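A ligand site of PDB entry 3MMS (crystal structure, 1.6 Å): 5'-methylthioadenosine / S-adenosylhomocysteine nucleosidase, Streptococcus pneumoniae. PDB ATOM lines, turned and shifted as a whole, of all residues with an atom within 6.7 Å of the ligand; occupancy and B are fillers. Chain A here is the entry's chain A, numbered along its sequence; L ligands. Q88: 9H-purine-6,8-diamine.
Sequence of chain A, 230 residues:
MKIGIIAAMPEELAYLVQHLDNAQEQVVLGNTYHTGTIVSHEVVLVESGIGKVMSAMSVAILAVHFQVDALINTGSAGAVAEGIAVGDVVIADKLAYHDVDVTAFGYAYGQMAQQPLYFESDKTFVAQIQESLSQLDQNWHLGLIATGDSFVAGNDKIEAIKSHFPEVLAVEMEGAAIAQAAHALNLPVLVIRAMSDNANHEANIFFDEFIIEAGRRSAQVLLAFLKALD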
ATOM      1  N   GLU A  12      10.169  23.659  14.116  1.00  0.00           N
ATOM      2  CA  GLU A  12      10.142  22.355  13.467  1.00  0.00           C
ATOM      3  C   GLU A  12       8.755  21.927  13.041  1.00  0.00           C
ATOM      4  O   GLU A  12       8.612  20.919  12.313  1.00  0.00           O
ATOM      5  CB  GLU A  12      10.770  21.317  14.418  1.00  0.00           C
ATOM      6  CG  GLU A  12      12.219  21.628  14.799  1.00  0.00           C
ATOM      7  CD  GLU A  12      12.723  20.801  15.962  1.00  0.00           C
ATOM      8  OE1 GLU A  12      11.890  20.419  16.808  1.00  0.00           O
ATOM      9  OE2 GLU A  12      13.942  20.556  16.053  1.00  0.00           O
ATOM     10  N   GLY A  75      12.256  17.083  12.860  1.00  0.00           N
ATOM     11  CA  GLY A  75      12.953  18.191  13.476  1.00  0.00           C
ATOM     12  C   GLY A  75      14.427  18.259  13.153  1.00  0.00           C
ATOM     13  O   GLY A  75      14.907  17.729  12.143  1.00  0.00           O
ATOM     14  N   SER A  76      15.151  18.920  14.038  1.00  0.00           N
ATOM     15  CA  SER A  76      16.583  19.126  13.880  1.00  0.00           C
ATOM     16  C   SER A  76      17.396  18.281  14.846  1.00  0.00           C
ATOM     17  O   SER A  76      16.932  17.885  15.909  1.00  0.00           O
ATOM     18  CB  SER A  76      16.898  20.617  14.115  1.00  0.00           C
ATOM     19  OG  SER A  76      16.589  20.977  15.456  1.00  0.00           O
ATOM     20  N   ALA A  77      18.646  17.998  14.463  1.00  0.00           N
ATOM     21  CA  ALA A  77      19.545  17.231  15.322  1.00  0.00           C
ATOM     22  C   ALA A  77      20.978  17.679  15.060  1.00  0.00           C
ATOM     23  O   ALA A  77      21.238  18.460  14.122  1.00  0.00           O
ATOM     24  CB  ALA A  77      19.413  15.701  15.035  1.00  0.00           C
ATOM     25  N   GLY A  78      21.897  17.174  15.881  1.00  0.00           N
ATOM     26  CA  GLY A  78      23.314  17.503  15.734  1.00  0.00           C
ATOM     27  C   GLY A  78      24.024  16.373  15.020  1.00  0.00           C
ATOM     28  O   GLY A  78      23.861  15.198  15.393  1.00  0.00           O
ATOM     29  N   ALA A  79      24.806  16.741  13.998  1.00  0.00           N
ATOM     30  CA  ALA A  79      25.561  15.784  13.173  1.00  0.00           C
ATOM     31  C   ALA A  79      26.863  15.354  13.823  1.00  0.00           C
ATOM     32  O   ALA A  79      27.705  16.212  14.163  1.00  0.00           O
ATOM     33  CB  ALA A  79      25.854  16.430  11.821  1.00  0.00           C
ATOM     34  N   HIS A  98      21.622   7.546  24.778  1.00  0.00           N
ATOM     35  CA  HIS A  98      23.044   7.590  25.065  1.00  0.00           C
ATOM     36  C   HIS A  98      23.302   7.955  26.531  1.00  0.00           C
ATOM     37  O   HIS A  98      24.446   7.918  26.970  1.00  0.00           O
ATOM     38  CB  HIS A  98      23.773   8.601  24.137  1.00  0.00           C
ATOM     39  CG  HIS A  98      23.333  10.035  24.285  1.00  0.00           C
ATOM     40  ND1 HIS A  98      23.632  10.802  25.390  1.00  0.00           N
ATOM     41  CD2 HIS A  98      22.677  10.848  23.417  1.00  0.00           C
ATOM     42  CE1 HIS A  98      23.173  12.024  25.206  1.00  0.00           C
ATOM     43  NE2 HIS A  98      22.593  12.087  24.013  1.00  0.00           N
ATOM     44  N   GLY A 148      19.209  11.755  24.212  1.00  0.00           N
ATOM     45  CA  GLY A 148      19.524  12.049  25.595  1.00  0.00           C
ATOM     46  C   GLY A 148      18.873  13.340  26.055  1.00  0.00           C
ATOM     47  O   GLY A 148      18.602  14.220  25.242  1.00  0.00           O
ATOM     48  N   SER A 150      19.851  15.972  27.044  1.00  0.00           N
ATOM     49  CA  SER A 150      20.973  16.896  27.098  1.00  0.00           C
ATOM     50  C   SER A 150      21.194  17.452  25.711  1.00  0.00           C
ATOM     51  O   SER A 150      21.037  16.744  24.715  1.00  0.00           O
ATOM     52  CB  SER A 150      22.284  16.283  27.605  1.00  0.00           C
ATOM     53  OG  SER A 150      22.221  15.970  28.979  1.00  0.00           O
ATOM     54  N   PHE A 151      21.589  18.712  25.634  1.00  0.00           N
ATOM     55  CA  PHE A 151      21.932  19.303  24.356  1.00  0.00           C
ATOM     56  C   PHE A 151      23.431  19.101  24.281  1.00  0.00           C
ATOM     57  O   PHE A 151      24.176  19.583  25.134  1.00  0.00           O
ATOM     58  CB  PHE A 151      21.592  20.791  24.324  1.00  0.00           C
ATOM     59  CG  PHE A 151      21.861  21.426  22.996  1.00  0.00           C
ATOM     60  CD1 PHE A 151      20.899  21.391  21.976  1.00  0.00           C
ATOM     61  CD2 PHE A 151      23.098  22.006  22.732  1.00  0.00           C
ATOM     62  CE1 PHE A 151      21.189  21.940  20.716  1.00  0.00           C
ATOM     63  CE2 PHE A 151      23.387  22.551  21.482  1.00  0.00           C
ATOM     64  CZ  PHE A 151      22.422  22.509  20.479  1.00  0.00           C
ATOM     65  N   VAL A 152      23.888  18.359  23.263  1.00  0.00           N
ATOM     66  CA  VAL A 152      25.315  18.021  23.103  1.00  0.00           C
ATOM     67  C   VAL A 152      26.062  19.186  22.463  1.00  0.00           C
ATOM     68  O   VAL A 152      25.740  19.611  21.362  1.00  0.00           O
ATOM     69  CB  VAL A 152      25.446  16.735  22.238  1.00  0.00           C
ATOM     70  CG1 VAL A 152      26.915  16.292  22.142  1.00  0.00           C
ATOM     71  CG2 VAL A 152      24.608  15.596  22.873  1.00  0.00           C
ATOM     72  N   ALA A 153      27.075  19.681  23.168  1.00  0.00           N
ATOM     73  CA  ALA A 153      27.816  20.844  22.678  1.00  0.00           C
ATOM     74  C   ALA A 153      29.269  20.755  23.103  1.00  0.00           C
ATOM     75  O   ALA A 153      29.765  21.599  23.869  1.00  0.00           O
ATOM     76  CB  ALA A 153      27.192  22.118  23.222  1.00  0.00           C
ATOM     77  N   VAL A 171      22.632  13.210  17.093  1.00  0.00           N
ATOM     78  CA  VAL A 171      22.163  13.231  18.475  1.00  0.00           C
ATOM     79  C   VAL A 171      21.078  14.272  18.663  1.00  0.00           C
ATOM     80  O   VAL A 171      21.119  15.346  18.071  1.00  0.00           O
ATOM     81  CB  VAL A 171      23.308  13.523  19.449  1.00  0.00           C
ATOM     82  CG1 VAL A 171      24.354  12.423  19.384  1.00  0.00           C
ATOM     83  CG2 VAL A 171      23.933  14.876  19.142  1.00  0.00           C
ATOM     84  N   GLU A 172      20.100  13.952  19.510  1.00  0.00           N
ATOM     85  CA  GLU A 172      19.052  14.898  19.852  1.00  0.00           C
ATOM     86  C   GLU A 172      18.251  14.407  21.063  1.00  0.00           C
ATOM     87  O   GLU A 172      18.545  13.343  21.594  1.00  0.00           O
ATOM     88  CB  GLU A 172      18.067  15.082  18.694  1.00  0.00           C
ATOM     89  CG  GLU A 172      17.675  13.800  17.985  1.00  0.00           C
ATOM     90  CD  GLU A 172      16.770  12.946  18.847  1.00  0.00           C
ATOM     91  OE1 GLU A 172      15.580  13.269  18.931  1.00  0.00           O
ATOM     92  OE2 GLU A 172      17.273  11.981  19.449  1.00  0.00           O
ATOM     93  N   MET A 173      17.284  15.189  21.496  1.00  0.00           N
ATOM     94  CA  MET A 173      16.655  14.929  22.789  1.00  0.00           C
ATOM     95  C   MET A 173      15.288  14.239  22.883  1.00  0.00           C
ATOM     96  O   MET A 173      14.721  14.168  23.965  1.00  0.00           O
ATOM     97  CB  MET A 173      16.590  16.292  23.489  1.00  0.00           C
ATOM     98  CG  MET A 173      17.949  16.949  23.630  1.00  0.00           C
ATOM     99  SD  MET A 173      17.864  18.663  24.210  1.00  0.00           S
ATOM    100  CE  MET A 173      17.379  18.417  25.910  1.00  0.00           C
ATOM    101  N   GLU A 174      14.780  13.722  21.774  1.00  0.00           N
ATOM    102  CA  GLU A 174      13.450  13.130  21.813  1.00  0.00           C
ATOM    103  C   GLU A 174      13.223  11.812  21.095  1.00  0.00           C
ATOM    104  O   GLU A 174      12.353  11.052  21.501  1.00  0.00           O
ATOM    105  CB  GLU A 174      12.407  14.114  21.230  1.00  0.00           C
ATOM    106  CG  GLU A 174      12.251  15.424  21.993  1.00  0.00           C
ATOM    107  CD  GLU A 174      13.228  16.488  21.567  1.00  0.00           C
ATOM    108  OE1 GLU A 174      13.751  16.398  20.417  1.00  0.00           O
ATOM    109  OE2 GLU A 174      13.476  17.422  22.349  1.00  0.00           O
ATOM    110  N   ARG A 193      15.213  13.579  10.828  1.00  0.00           N
ATOM    111  CA  ARG A 193      15.864  14.797  11.339  1.00  0.00           C
ATOM    112  C   ARG A 193      16.711  15.437  10.256  1.00  0.00           C
ATOM    113  O   ARG A 193      17.197  14.762   9.355  1.00  0.00           O
ATOM    114  CB  ARG A 193      16.822  14.492  12.500  1.00  0.00           C
ATOM    115  CG  ARG A 193      16.151  14.100  13.823  1.00  0.00           C
ATOM    116  CD  ARG A 193      15.369  15.300  14.412  1.00  0.00           C
ATOM    117  NE  ARG A 193      14.838  14.973  15.738  1.00  0.00           N
ATOM    118  CZ  ARG A 193      13.746  14.231  15.954  1.00  0.00           C
ATOM    119  NH1 ARG A 193      13.027  13.755  14.945  1.00  0.00           N
ATOM    120  NH2 ARG A 193      13.421  13.920  17.200  1.00  0.00           N
ATOM    121  N   ALA A 194      16.874  16.757  10.338  1.00  0.00           N
ATOM    122  CA  ALA A 194      17.811  17.448   9.431  1.00  0.00           C
ATOM    123  C   ALA A 194      18.870  18.061  10.383  1.00  0.00           C
ATOM    124  O   ALA A 194      18.528  18.481  11.492  1.00  0.00           O
ATOM    125  CB  ALA A 194      17.134  18.530   8.640  1.00  0.00           C
ATOM    126  N   MET A 195      20.119  18.128   9.948  1.00  0.00           N
ATOM    127  CA  MET A 195      21.209  18.609  10.801  1.00  0.00           C
ATOM    128  C   MET A 195      21.332  20.118  10.851  1.00  0.00           C
ATOM    129  O   MET A 195      21.429  20.770   9.816  1.00  0.00           O
ATOM    130  CB  MET A 195      22.556  18.019  10.317  1.00  0.00           C
ATOM    131  CG  MET A 195      22.522  16.492  10.102  1.00  0.00           C
ATOM    132  SD  MET A 195      22.173  15.488  11.601  1.00  0.00           S
ATOM    133  CE  MET A 195      20.411  15.104  11.402  1.00  0.00           C
ATOM    134  N   SER A 196      21.312  20.652  12.077  1.00  0.00           N
ATOM    135  CA  SER A 196      21.443  22.101  12.267  1.00  0.00           C
ATOM    136  C   SER A 196      22.822  22.496  12.809  1.00  0.00           C
ATOM    137  O   SER A 196      23.177  23.685  12.797  1.00  0.00           O
ATOM    138  CB  SER A 196      20.407  22.615  13.269  1.00  0.00           C
ATOM    139  OG  SER A 196      20.541  21.923  14.499  1.00  0.00           O
ATOM    140  N   ASP A 197      23.577  21.530  13.300  1.00  0.00           N
ATOM    141  CA  ASP A 197      24.855  21.829  13.908  1.00  0.00           C
ATOM    142  C   ASP A 197      25.673  20.548  14.019  1.00  0.00           C
ATOM    143  O   ASP A 197      25.216  19.476  13.595  1.00  0.00           O
ATOM    144  CB  ASP A 197      24.628  22.445  15.327  1.00  0.00           C
ATOM    145  CG  ASP A 197      23.846  21.537  16.253  1.00  0.00           C
ATOM    146  OD1 ASP A 197      24.476  20.688  16.919  1.00  0.00           O
ATOM    147  OD2 ASP A 197      22.598  21.656  16.294  1.00  0.00           O
ATOM    148  N   ASN A 198      26.871  20.657  14.598  1.00  0.00           N
ATOM    149  CA  ASN A 198      27.773  19.527  14.725  1.00  0.00           C
ATOM    150  C   ASN A 198      27.916  19.048  16.167  1.00  0.00           C
ATOM    151  O   ASN A 198      28.807  18.276  16.482  1.00  0.00           O
ATOM    152  CB  ASN A 198      29.147  19.887  14.162  1.00  0.00           C
ATOM    153  CG  ASN A 198      29.183  19.834  12.645  1.00  0.00           C
ATOM    154  OD1 ASN A 198      29.160  18.753  12.059  1.00  0.00           O
ATOM    155  ND2 ASN A 198      29.239  20.998  12.013  1.00  0.00           N
ATOM    156  N   ALA A 199      27.035  19.527  17.039  1.00  0.00           N
ATOM    157  CA  ALA A 199      27.034  19.085  18.429  1.00  0.00           C
ATOM    158  C   ALA A 199      28.383  19.333  19.105  1.00  0.00           C
ATOM    159  O   ALA A 199      28.724  18.669  20.076  1.00  0.00           O
ATOM    160  CB  ALA A 199      26.673  17.621  18.520  1.00  0.00           C
ATOM    161  N   ASN A 200      29.133  20.301  18.597  1.00  0.00           N
ATOM    162  CA  ASN A 200      30.431  20.642  19.149  1.00  0.00           C
ATOM    163  C   ASN A 200      30.375  21.879  20.051  1.00  0.00           C
ATOM    164  O   ASN A 200      29.305  22.274  20.494  1.00  0.00           O
ATOM    165  CB  ASN A 200      31.445  20.871  18.035  1.00  0.00           C
ATOM    166  CG  ASN A 200      31.010  21.959  17.080  1.00  0.00           C
ATOM    167  OD1 ASN A 200      30.141  22.757  17.406  1.00  0.00           O
ATOM    168  ND2 ASN A 200      31.615  21.993  15.903  1.00  0.00           N
ATOM    169  N   ALA A 203      27.840  24.480  19.149  1.00  0.00           N
ATOM    170  CA  ALA A 203      26.604  23.862  18.697  1.00  0.00           C
ATOM    171  C   ALA A 203      25.407  24.779  18.906  1.00  0.00           C
ATOM    172  O   ALA A 203      24.526  24.875  18.045  1.00  0.00           O
ATOM    173  CB  ALA A 203      26.389  22.529  19.401  1.00  0.00           C
ATOM    174  N   ASN A 204      25.367  25.448  20.050  1.00  0.00           N
ATOM    175  CA  ASN A 204      24.255  26.336  20.360  1.00  0.00           C
ATOM    176  C   ASN A 204      24.185  27.516  19.390  1.00  0.00           C
ATOM    177  O   ASN A 204      23.102  27.988  19.060  1.00  0.00           O
ATOM    178  CB  ASN A 204      24.331  26.832  21.803  1.00  0.00           C
ATOM    179  CG  ASN A 204      25.620  27.587  22.099  1.00  0.00           C
ATOM    180  OD1 ASN A 204      25.608  28.803  22.276  1.00  0.00           O
ATOM    181  ND2 ASN A 204      26.725  26.861  22.163  1.00  0.00           N
ATOM    182  N   PHE A 207      22.977  26.031  15.987  1.00  0.00           N
ATOM    183  CA  PHE A 207      21.588  25.629  16.165  1.00  0.00           C
ATOM    184  C   PHE A 207      20.719  26.903  16.000  1.00  0.00           C
ATOM    185  O   PHE A 207      19.732  26.910  15.240  1.00  0.00           O
ATOM    186  CB  PHE A 207      21.385  25.056  17.570  1.00  0.00           C
ATOM    187  CG  PHE A 207      19.940  24.840  17.927  1.00  0.00           C
ATOM    188  CD1 PHE A 207      19.186  25.868  18.499  1.00  0.00           C
ATOM    189  CD2 PHE A 207      19.330  23.613  17.658  1.00  0.00           C
ATOM    190  CE1 PHE A 207      17.841  25.691  18.801  1.00  0.00           C
ATOM    191  CE2 PHE A 207      17.975  23.414  17.961  1.00  0.00           C
ATOM    192  CZ  PHE A 207      17.221  24.455  18.526  1.00  0.00           C
ATOM    193  N   ILE A 211      18.249  26.546  12.855  1.00  0.00           N
ATOM    194  CA  ILE A 211      17.070  25.805  13.283  1.00  0.00           C
ATOM    195  C   ILE A 211      15.920  25.909  12.275  1.00  0.00           C
ATOM    196  O   ILE A 211      15.269  24.907  11.965  1.00  0.00           O
ATOM    197  CB  ILE A 211      16.640  26.243  14.732  1.00  0.00           C
ATOM    198  CG1 ILE A 211      15.354  25.547  15.128  1.00  0.00           C
ATOM    199  CG2 ILE A 211      16.484  27.749  14.811  1.00  0.00           C
ATOM    200  CD1 ILE A 211      15.485  24.050  15.134  1.00  0.00           C
ATOM    201  N   ALA A 214      16.750  23.750   9.169  1.00  0.00           N
ATOM    202  CA  ALA A 214      16.712  22.333   9.503  1.00  0.00           C
ATOM    203  C   ALA A 214      15.286  21.868   9.726  1.00  0.00           C
ATOM    204  O   ALA A 214      14.889  20.800   9.248  1.00  0.00           O
ATOM    205  CB  ALA A 214      17.606  22.039  10.734  1.00  0.00           C
HETATM  206  N1  Q88 L   1      22.137  18.151  20.883  1.00  0.00           N
HETATM  207  C2  Q88 L   1      20.909  17.771  21.246  1.00  0.00           C
HETATM  208  N3  Q88 L   1      19.828  18.059  20.512  1.00  0.00           N
HETATM  209  C4  Q88 L   1      19.942  18.762  19.369  1.00  0.00           C
HETATM  210  C5  Q88 L   1      21.233  19.198  18.929  1.00  0.00           C
HETATM  211  C6  Q88 L   1      22.360  18.870  19.753  1.00  0.00           C
HETATM  212  N6  Q88 L   1      23.654  19.246  19.420  1.00  0.00           N
HETATM  213  N7  Q88 L   1      21.036  19.892  17.766  1.00  0.00           N
HETATM  214  C8  Q88 L   1      19.734  19.877  17.488  1.00  0.00           C
HETATM  215  N8  Q88 L   1      19.130  20.461  16.412  1.00  0.00           N
HETATM  216  N9  Q88 L   1      19.053  19.202  18.443  1.00  0.00           N
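O of Ser 76 lies close to N8 of the ligand, at 3.4 Å.
The backbone NH (N) of Gly 78 is in hydrogen-bond range of a nitrogen (N7) of the ligand (3.4 Å).
A nitrogen (N8) of the ligand sits at hydrogen-bond distance from the side-chain hydroxyl (OG) of Ser 196, at 2.8 Å.
The backbone carbonyl oxygen of Val 152 is in hydrogen-bond range of a nitrogen (N6) of the ligand (2.9 Å).
A nitrogen (N7) of the ligand lies within hydrogen-bond range of the side-chain carboxylate (OD2) of Asp 197.
A nitrogen (N1) of the ligand sits at hydrogen-bond distance from the backbone NH (N) of Val 152 (3.0 Å).
A nitrogen (N8) of the ligand is in hydrogen-bond range of the side-chain hydroxyl of Ser 76.
The side-chain carboxylate of Glu 172 is in salt-bridge range of the guanidinium group of Arg 193 (2.8 Å).
The backbone carbonyl oxygen (O) of Glu 172 sits at hydrogen-bond distance from the backbone NH (N) of Gly 148, at 3.1 Å.
The backbone carbonyl oxygen of Ala 194 lies within hydrogen-bond range of the backbone NH of Ala 77 (3.0 Å).
O of Asp 197 is in hydrogen-bond range of N of Ala 79.
N of Ser 196 sits at hydrogen-bond distance from O of Ala 77 (3.0 Å).
The side-chain carboxylate (OD1) of Asp 197 sits at hydrogen-bond distance from the backbone NH (N) of Ala 199, 2.8 Å away.
The side-chain hydroxyl (OG) of Ser 76 sits at hydrogen-bond distance from the side-chain carboxylate (OE2) of Glu 12, 2.7 Å away.
The side-chain carboxylate (OE1) of Glu 172 is in hydrogen-bond range of the backbone NH (N) of Glu 174.
The backbone NH (N) of Ala 77 lies close to a nitrogen (N8) of the ligand.
O of Ser 150 touches C2 of the ligand, at 3.6 Å.
Phe 151 touches the ligand (CE1 to C5, 3.3 Å).
Val 171 touches the ligand (O to C4, 3.8 Å).
Glu 172 touches the ligand (CA to N3, 3.3 Å).
CG of Met 173 touches N3 of the ligand, 3.8 Å away.
Ala 199 touches the ligand (CA to N6, 3.5 Å).
Phe 207 touches the ligand (CD2 to N8, 3.4 Å).
Hydrophobic or aromatic side chains that line the ligand: Phe 151, Val 152, Met 173, Ala 199 and Phe 207.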
